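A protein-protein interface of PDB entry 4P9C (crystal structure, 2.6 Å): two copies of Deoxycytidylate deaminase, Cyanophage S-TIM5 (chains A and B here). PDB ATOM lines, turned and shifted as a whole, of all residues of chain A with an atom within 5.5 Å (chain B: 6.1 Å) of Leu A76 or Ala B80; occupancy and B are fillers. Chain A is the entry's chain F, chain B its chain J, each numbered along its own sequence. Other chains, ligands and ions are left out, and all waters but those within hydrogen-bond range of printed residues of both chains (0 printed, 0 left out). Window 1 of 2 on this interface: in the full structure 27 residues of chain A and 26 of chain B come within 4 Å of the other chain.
Of the printed residues of chain A, Ser B82 touches Glu A84 and Ser A85.
Of the printed residues of chain A, Glu B84 touches Ala A80.
The nearest residue of chain B that does not touch Leu A76 is Val B77 (4.2 Å).
The nearest residue of chain A that does not touch Ala B80 is Asp A87 (4.8 Å).
The side-chain hydroxyl of Ser A85 lies within hydrogen-bond range of the backbone carbonyl oxygen of Lys B81.
N of Ile A86 lies within hydrogen-bond range of O of Ala B80, 2.8 Å away.
O of Ser B82 lies close to O of Glu A84, at 3.2 Å.
Among the printed residues, merely in contact across the chains: Leu A76 with Ala B80, Met A79 with Met B79, Met A79 with Ala B80, Ala A80 with Met B79, Ala A80 with Ala B80, Ala A80 with Glu B84, Glu A84 with Ala B80, Ser A85 with Ala B80, Ser A85 with Ser B82, Ile A86 with Lys B81, Asp A87 with Lys B81, Met A104 with Val B77, Ala A108 with Val B77 and Ala A108 with Lys B81.
Hydrophobic or aromatic side chains of chain A within 4 Å of the printed part of chain B: Leu A76, Met A79, Ala A80, Ile A86 and Met A104.
Among the printed residues, 17 pairs touch across the chains.
Among the printed residues, no Asp or Glu carboxylate lies within 4 Å of a Lys or Arg side-chain nitrogen of the other chain.
The side-chain hydroxyl of Ser A85 lies within hydrogen-bond range of the backbone NH of Asp A87 (3.2 Å).
The side-chain hydroxyl of Ser B82 is in hydrogen-bond range of the backbone NH of Glu B84, at 3.2 Å.
Leu A76 touches Ala B80, but with the chains exchanged Ala A80 does not touch Leu B76 (4.1 Å).
Met A79 touches Ala B80, and with the chains exchanged Ala A80 touches Met B79.
Ala A80 touches its own counterpart, Ala B80.
Ala A80 touches Glu B84, and with the chains exchanged Glu A84 touches Ala B80.
8 positions are printed for both chains.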
ATOM      1  N   ALA A  71      10.203   5.899 -20.301  1.00  0.00           N
ATOM      2  CA  ALA A  71      11.560   5.353 -20.273  1.00  0.00           C
ATOM      3  C   ALA A  71      12.627   6.425 -20.520  1.00  0.00           C
ATOM      4  O   ALA A  71      13.709   6.367 -19.936  1.00  0.00           O
ATOM      5  CB  ALA A  71      11.699   4.225 -21.282  1.00  0.00           C
ATOM      6  N   GLU A  72      12.311   7.396 -21.381  1.00  0.00           N
ATOM      7  CA  GLU A  72      13.230   8.501 -21.687  1.00  0.00           C
ATOM      8  C   GLU A  72      13.365   9.466 -20.514  1.00  0.00           C
ATOM      9  O   GLU A  72      14.457   9.971 -20.246  1.00  0.00           O
ATOM     10  CB  GLU A  72      12.788   9.272 -22.935  1.00  0.00           C
ATOM     11  CG  GLU A  72      12.649   8.433 -24.203  1.00  0.00           C
ATOM     12  CD  GLU A  72      11.315   7.706 -24.289  1.00  0.00           C
ATOM     13  OE1 GLU A  72      11.199   6.787 -25.125  1.00  0.00           O
ATOM     14  OE2 GLU A  72      10.380   8.048 -23.530  1.00  0.00           O
ATOM     15  N   GLN A  73      12.249   9.729 -19.827  1.00  0.00           N
ATOM     16  CA  GLN A  73      12.237  10.579 -18.632  1.00  0.00           C
ATOM     17  C   GLN A  73      13.093   9.980 -17.524  1.00  0.00           C
ATOM     18  O   GLN A  73      13.951  10.659 -16.961  1.00  0.00           O
ATOM     19  CB  GLN A  73      10.811  10.767 -18.102  1.00  0.00           C
ATOM     20  CG  GLN A  73       9.996  11.860 -18.775  1.00  0.00           C
ATOM     21  CD  GLN A  73       8.608  12.002 -18.160  1.00  0.00           C
ATOM     22  OE1 GLN A  73       7.857  11.031 -18.061  1.00  0.00           O
ATOM     23  NE2 GLN A  73       8.265  13.216 -17.749  1.00  0.00           N
ATOM     24  N   ASN A  74      12.839   8.708 -17.217  1.00  0.00           N
ATOM     25  CA  ASN A  74      13.589   7.990 -16.193  1.00  0.00           C
ATOM     26  C   ASN A  74      15.085   7.939 -16.504  1.00  0.00           C
ATOM     27  O   ASN A  74      15.912   8.030 -15.595  1.00  0.00           O
ATOM     28  CB  ASN A  74      13.014   6.584 -15.982  1.00  0.00           C
ATOM     29  CG  ASN A  74      11.852   6.562 -14.986  1.00  0.00           C
ATOM     30  OD1 ASN A  74      11.877   7.248 -13.961  1.00  0.00           O
ATOM     31  ND2 ASN A  74      10.837   5.756 -15.280  1.00  0.00           N
ATOM     32  N   ALA A  75      15.420   7.806 -17.787  1.00  0.00           N
ATOM     33  CA  ALA A  75      16.811   7.839 -18.237  1.00  0.00           C
ATOM     34  C   ALA A  75      17.426   9.217 -18.017  1.00  0.00           C
ATOM     35  O   ALA A  75      18.583   9.330 -17.599  1.00  0.00           O
ATOM     36  CB  ALA A  75      16.910   7.440 -19.702  1.00  0.00           C
ATOM     37  N   LEU A  76      16.643  10.256 -18.293  1.00  0.00           N
ATOM     38  CA  LEU A  76      17.061  11.630 -18.061  1.00  0.00           C
ATOM     39  C   LEU A  76      17.211  11.888 -16.559  1.00  0.00           C
ATOM     40  O   LEU A  76      18.202  12.478 -16.124  1.00  0.00           O
ATOM     41  CB  LEU A  76      16.030  12.591 -18.656  1.00  0.00           C
ATOM     42  CG  LEU A  76      16.473  13.756 -19.553  1.00  0.00           C
ATOM     43  CD1 LEU A  76      17.421  14.722 -18.847  1.00  0.00           C
ATOM     44  CD2 LEU A  76      17.065  13.262 -20.877  1.00  0.00           C
ATOM     45  N   VAL A  77      16.224  11.437 -15.782  1.00  0.00           N
ATOM     46  CA  VAL A  77      16.199  11.633 -14.323  1.00  0.00           C
ATOM     47  C   VAL A  77      17.365  10.902 -13.659  1.00  0.00           C
ATOM     48  O   VAL A  77      18.008  11.442 -12.754  1.00  0.00           O
ATOM     49  CB  VAL A  77      14.842  11.193 -13.701  1.00  0.00           C
ATOM     50  CG1 VAL A  77      14.946  11.013 -12.194  1.00  0.00           C
ATOM     51  CG2 VAL A  77      13.746  12.198 -14.039  1.00  0.00           C
ATOM     52  N   LYS A  78      17.631   9.684 -14.127  1.00  0.00           N
ATOM     53  CA  LYS A  78      18.786   8.920 -13.672  1.00  0.00           C
ATOM     54  C   LYS A  78      20.107   9.661 -13.916  1.00  0.00           C
ATOM     55  O   LYS A  78      20.977   9.675 -13.043  1.00  0.00           O
ATOM     56  CB  LYS A  78      18.818   7.529 -14.322  1.00  0.00           C
ATOM     57  CG  LYS A  78      19.821   6.560 -13.698  1.00  0.00           C
ATOM     58  CD  LYS A  78      19.408   6.124 -12.292  1.00  0.00           C
ATOM     59  CE  LYS A  78      20.562   5.462 -11.553  1.00  0.00           C
ATOM     60  NZ  LYS A  78      20.136   4.879 -10.245  1.00  0.00           N
ATOM     61  N   MET A  79      20.245  10.279 -15.091  1.00  0.00           N
ATOM     62  CA  MET A  79      21.469  10.998 -15.453  1.00  0.00           C
ATOM     63  C   MET A  79      21.679  12.267 -14.625  1.00  0.00           C
ATOM     64  O   MET A  79      22.809  12.743 -14.480  1.00  0.00           O
ATOM     65  CB  MET A  79      21.498  11.319 -16.951  1.00  0.00           C
ATOM     66  CG  MET A  79      21.767  10.109 -17.847  1.00  0.00           C
ATOM     67  SD  MET A  79      23.298   9.227 -17.452  1.00  0.00           S
ATOM     68  CE  MET A  79      24.540  10.470 -17.823  1.00  0.00           C
ATOM     69  N   ALA A  80      20.585  12.798 -14.086  1.00  0.00           N
ATOM     70  CA  ALA A  80      20.645  13.917 -13.154  1.00  0.00           C
ATOM     71  C   ALA A  80      21.125  13.474 -11.767  1.00  0.00           C
ATOM     72  O   ALA A  80      21.794  14.239 -11.069  1.00  0.00           O
ATOM     73  CB  ALA A  80      19.289  14.599 -13.060  1.00  0.00           C
ATOM     74  N   LYS A  81      20.778  12.244 -11.375  1.00  0.00           N
ATOM     75  CA  LYS A  81      21.242  11.668 -10.108  1.00  0.00           C
ATOM     76  C   LYS A  81      22.659  11.139 -10.243  1.00  0.00           C
ATOM     77  O   LYS A  81      23.357  10.938  -9.241  1.00  0.00           O
ATOM     78  CB  LYS A  81      20.351  10.512  -9.652  1.00  0.00           C
ATOM     79  CG  LYS A  81      18.864  10.803  -9.575  1.00  0.00           C
ATOM     80  CD  LYS A  81      18.302  10.112  -8.326  1.00  0.00           C
ATOM     81  CE  LYS A  81      17.116   9.213  -8.715  1.00  0.00           C
ATOM     82  NZ  LYS A  81      16.441   8.679  -7.471  1.00  0.00           N
ATOM     83  N   GLU A  84      27.831  11.575 -13.849  1.00  0.00           N
ATOM     84  CA  GLU A  84      28.344  11.644 -15.214  1.00  0.00           C
ATOM     85  C   GLU A  84      27.438  12.536 -16.066  1.00  0.00           C
ATOM     86  O   GLU A  84      26.244  12.681 -15.780  1.00  0.00           O
ATOM     87  CB  GLU A  84      28.477  10.238 -15.818  1.00  0.00           C
ATOM     88  CG  GLU A  84      29.365  10.152 -17.067  1.00  0.00           C
ATOM     89  CD  GLU A  84      30.828  10.476 -16.796  1.00  0.00           C
ATOM     90  OE1 GLU A  84      31.396   9.944 -15.818  1.00  0.00           O
ATOM     91  OE2 GLU A  84      31.414  11.261 -17.573  1.00  0.00           O
ATOM     92  N   SER A  85      28.018  13.141 -17.107  1.00  0.00           N
ATOM     93  CA  SER A  85      27.292  14.073 -17.972  1.00  0.00           C
ATOM     94  C   SER A  85      26.611  13.361 -19.134  1.00  0.00           C
ATOM     95  O   SER A  85      27.169  12.429 -19.717  1.00  0.00           O
ATOM     96  CB  SER A  85      28.239  15.154 -18.510  1.00  0.00           C
ATOM     97  OG  SER A  85      27.569  16.039 -19.394  1.00  0.00           O
ATOM     98  N   ILE A  86      25.407  13.816 -19.464  1.00  0.00           N
ATOM     99  CA  ILE A  86      24.650  13.256 -20.579  1.00  0.00           C
ATOM    100  C   ILE A  86      25.035  13.936 -21.897  1.00  0.00           C
ATOM    101  O   ILE A  86      24.716  13.435 -22.978  1.00  0.00           O
ATOM    102  CB  ILE A  86      23.120  13.330 -20.326  1.00  0.00           C
ATOM    103  CG1 ILE A  86      22.376  12.310 -21.201  1.00  0.00           C
ATOM    104  CG2 ILE A  86      22.598  14.762 -20.514  1.00  0.00           C
ATOM    105  CD1 ILE A  86      20.913  12.053 -20.760  1.00  0.00           C
ATOM    106  N   ASP A  87      25.726  15.071 -21.795  1.00  0.00           N
ATOM    107  CA  ASP A  87      26.171  15.824 -22.967  1.00  0.00           C
ATOM    108  C   ASP A  87      27.096  14.978 -23.851  1.00  0.00           C
ATOM    109  O   ASP A  87      28.080  14.415 -23.372  1.00  0.00           O
ATOM    110  CB  ASP A  87      26.885  17.108 -22.536  1.00  0.00           C
ATOM    111  CG  ASP A  87      27.001  18.129 -23.660  1.00  0.00           C
ATOM    112  OD1 ASP A  87      26.186  18.089 -24.607  1.00  0.00           O
ATOM    113  OD2 ASP A  87      27.911  18.982 -23.589  1.00  0.00           O
ATOM    114  N   MET A 104      13.385  17.649 -24.136  1.00  0.00           N
ATOM    115  CA  MET A 104      14.397  17.573 -23.078  1.00  0.00           C
ATOM    116  C   MET A 104      15.664  16.851 -23.544  1.00  0.00           C
ATOM    117  O   MET A 104      16.778  17.249 -23.191  1.00  0.00           O
ATOM    118  CB  MET A 104      13.825  16.904 -21.822  1.00  0.00           C
ATOM    119  CG  MET A 104      12.762  17.730 -21.102  1.00  0.00           C
ATOM    120  SD  MET A 104      12.102  16.931 -19.619  1.00  0.00           S
ATOM    121  CE  MET A 104      11.130  15.604 -20.334  1.00  0.00           C
ATOM    122  N   ILE A 105      15.481  15.797 -24.341  1.00  0.00           N
ATOM    123  CA  ILE A 105      16.591  15.014 -24.900  1.00  0.00           C
ATOM    124  C   ILE A 105      17.535  15.885 -25.742  1.00  0.00           C
ATOM    125  O   ILE A 105      18.760  15.778 -25.618  1.00  0.00           O
ATOM    126  CB  ILE A 105      16.069  13.793 -25.713  1.00  0.00           C
ATOM    127  CG1 ILE A 105      15.487  12.738 -24.763  1.00  0.00           C
ATOM    128  CG2 ILE A 105      17.172  13.175 -26.572  1.00  0.00           C
ATOM    129  CD1 ILE A 105      14.487  11.788 -25.416  1.00  0.00           C
ATOM    130  N   ALA A 108      19.399  18.318 -23.538  1.00  0.00           N
ATOM    131  CA  ALA A 108      20.386  17.586 -22.745  1.00  0.00           C
ATOM    132  C   ALA A 108      21.734  17.432 -23.460  1.00  0.00           C
ATOM    133  O   ALA A 108      22.766  17.255 -22.812  1.00  0.00           O
ATOM    134  CB  ALA A 108      19.834  16.224 -22.350  1.00  0.00           C
ATOM    135  N   ALA B  75      16.297  23.243 -15.367  1.00  0.00           N
ATOM    136  CA  ALA B  75      17.108  22.940 -14.192  1.00  0.00           C
ATOM    137  C   ALA B  75      17.427  21.447 -14.121  1.00  0.00           C
ATOM    138  O   ALA B  75      18.535  21.062 -13.744  1.00  0.00           O
ATOM    139  CB  ALA B  75      16.403  23.401 -12.923  1.00  0.00           C
ATOM    140  N   LEU B  76      16.450  20.619 -14.488  1.00  0.00           N
ATOM    141  CA  LEU B  76      16.583  19.164 -14.480  1.00  0.00           C
ATOM    142  C   LEU B  76      17.580  18.699 -15.544  1.00  0.00           C
ATOM    143  O   LEU B  76      18.513  17.950 -15.248  1.00  0.00           O
ATOM    144  CB  LEU B  76      15.207  18.525 -14.721  1.00  0.00           C
ATOM    145  CG  LEU B  76      14.780  17.185 -14.103  1.00  0.00           C
ATOM    146  CD1 LEU B  76      15.642  16.006 -14.560  1.00  0.00           C
ATOM    147  CD2 LEU B  76      14.704  17.249 -12.576  1.00  0.00           C
ATOM    148  N   VAL B  77      17.363  19.156 -16.776  1.00  0.00           N
ATOM    149  CA  VAL B  77      18.224  18.845 -17.918  1.00  0.00           C
ATOM    150  C   VAL B  77      19.668  19.275 -17.662  1.00  0.00           C
ATOM    151  O   VAL B  77      20.610  18.555 -18.001  1.00  0.00           O
ATOM    152  CB  VAL B  77      17.679  19.508 -19.209  1.00  0.00           C
ATOM    153  CG1 VAL B  77      18.764  19.665 -20.268  1.00  0.00           C
ATOM    154  CG2 VAL B  77      16.506  18.709 -19.760  1.00  0.00           C
ATOM    155  N   LYS B  78      19.821  20.452 -17.056  1.00  0.00           N
ATOM    156  CA  LYS B  78      21.128  20.983 -16.691  1.00  0.00           C
ATOM    157  C   LYS B  78      21.868  20.037 -15.745  1.00  0.00           C
ATOM    158  O   LYS B  78      23.074  19.833 -15.887  1.00  0.00           O
ATOM    159  CB  LYS B  78      20.974  22.371 -16.056  1.00  0.00           C
ATOM    160  CG  LYS B  78      22.284  23.094 -15.771  1.00  0.00           C
ATOM    161  CD  LYS B  78      22.978  23.526 -17.057  1.00  0.00           C
ATOM    162  CE  LYS B  78      24.434  23.879 -16.798  1.00  0.00           C
ATOM    163  NZ  LYS B  78      25.117  24.331 -18.042  1.00  0.00           N
ATOM    164  N   MET B  79      21.133  19.462 -14.794  1.00  0.00           N
ATOM    165  CA  MET B  79      21.704  18.514 -13.838  1.00  0.00           C
ATOM    166  C   MET B  79      22.155  17.202 -14.484  1.00  0.00           C
ATOM    167  O   MET B  79      23.088  16.560 -13.995  1.00  0.00           O
ATOM    168  CB  MET B  79      20.735  18.242 -12.684  1.00  0.00           C
ATOM    169  CG  MET B  79      20.594  19.402 -11.698  1.00  0.00           C
ATOM    170  SD  MET B  79      22.160  19.990 -11.011  1.00  0.00           S
ATOM    171  CE  MET B  79      22.713  18.565 -10.080  1.00  0.00           C
ATOM    172  N   ALA B  80      21.492  16.807 -15.570  1.00  0.00           N
ATOM    173  CA  ALA B  80      21.888  15.619 -16.329  1.00  0.00           C
ATOM    174  C   ALA B  80      23.164  15.875 -17.135  1.00  0.00           C
ATOM    175  O   ALA B  80      24.005  14.984 -17.291  1.00  0.00           O
ATOM    176  CB  ALA B  80      20.761  15.171 -17.241  1.00  0.00           C
ATOM    177  N   LYS B  81      23.291  17.102 -17.630  1.00  0.00           N
ATOM    178  CA  LYS B  81      24.452  17.562 -18.385  1.00  0.00           C
ATOM    179  C   LYS B  81      25.630  17.809 -17.443  1.00  0.00           C
ATOM    180  O   LYS B  81      26.779  17.922 -17.877  1.00  0.00           O
ATOM    181  CB  LYS B  81      24.081  18.859 -19.104  1.00  0.00           C
ATOM    182  CG  LYS B  81      24.717  19.049 -20.471  1.00  0.00           C
ATOM    183  CD  LYS B  81      23.882  19.988 -21.354  1.00  0.00           C
ATOM    184  CE  LYS B  81      24.048  21.451 -20.961  1.00  0.00           C
ATOM    185  NZ  LYS B  81      23.238  22.358 -21.822  1.00  0.00           N
ATOM    186  N   SER B  82      25.317  17.908 -16.154  1.00  0.00           N
ATOM    187  CA  SER B  82      26.299  18.186 -15.113  1.00  0.00           C
ATOM    188  C   SER B  82      26.998  16.907 -14.672  1.00  0.00           C
ATOM    189  O   SER B  82      26.597  15.804 -15.054  1.00  0.00           O
ATOM    190  CB  SER B  82      25.619  18.857 -13.913  1.00  0.00           C
ATOM    191  OG  SER B  82      26.567  19.199 -12.912  1.00  0.00           O
ATOM    192  N   SER B  83      28.046  17.064 -13.869  1.00  0.00           N
ATOM    193  CA  SER B  83      28.755  15.927 -13.301  1.00  0.00           C
ATOM    194  C   SER B  83      28.517  15.829 -11.794  1.00  0.00           C
ATOM    195  O   SER B  83      29.241  15.126 -11.086  1.00  0.00           O
ATOM    196  CB  SER B  83      30.249  16.012 -13.616  1.00  0.00           C
ATOM    197  OG  SER B  83      30.827  17.176 -13.044  1.00  0.00           O
ATOM    198  N   GLU B  84      27.505  16.541 -11.311  1.00  0.00           N
ATOM    199  CA  GLU B  84      27.113  16.467  -9.907  1.00  0.00           C
ATOM    200  C   GLU B  84      25.694  15.909  -9.788  1.00  0.00           C
ATOM    201  O   GLU B  84      24.914  15.959 -10.745  1.00  0.00           O
ATOM    202  CB  GLU B  84      27.254  17.839  -9.231  1.00  0.00           C
ATOM    203  CG  GLU B  84      27.054  17.852  -7.708  1.00  0.00           C
ATOM    204  CD  GLU B  84      28.193  17.198  -6.934  1.00  0.00           C
ATOM    205  OE1 GLU B  84      28.944  17.930  -6.256  1.00  0.00           O
ATOM    206  OE2 GLU B  84      28.332  15.959  -6.994  1.00  0.00           O
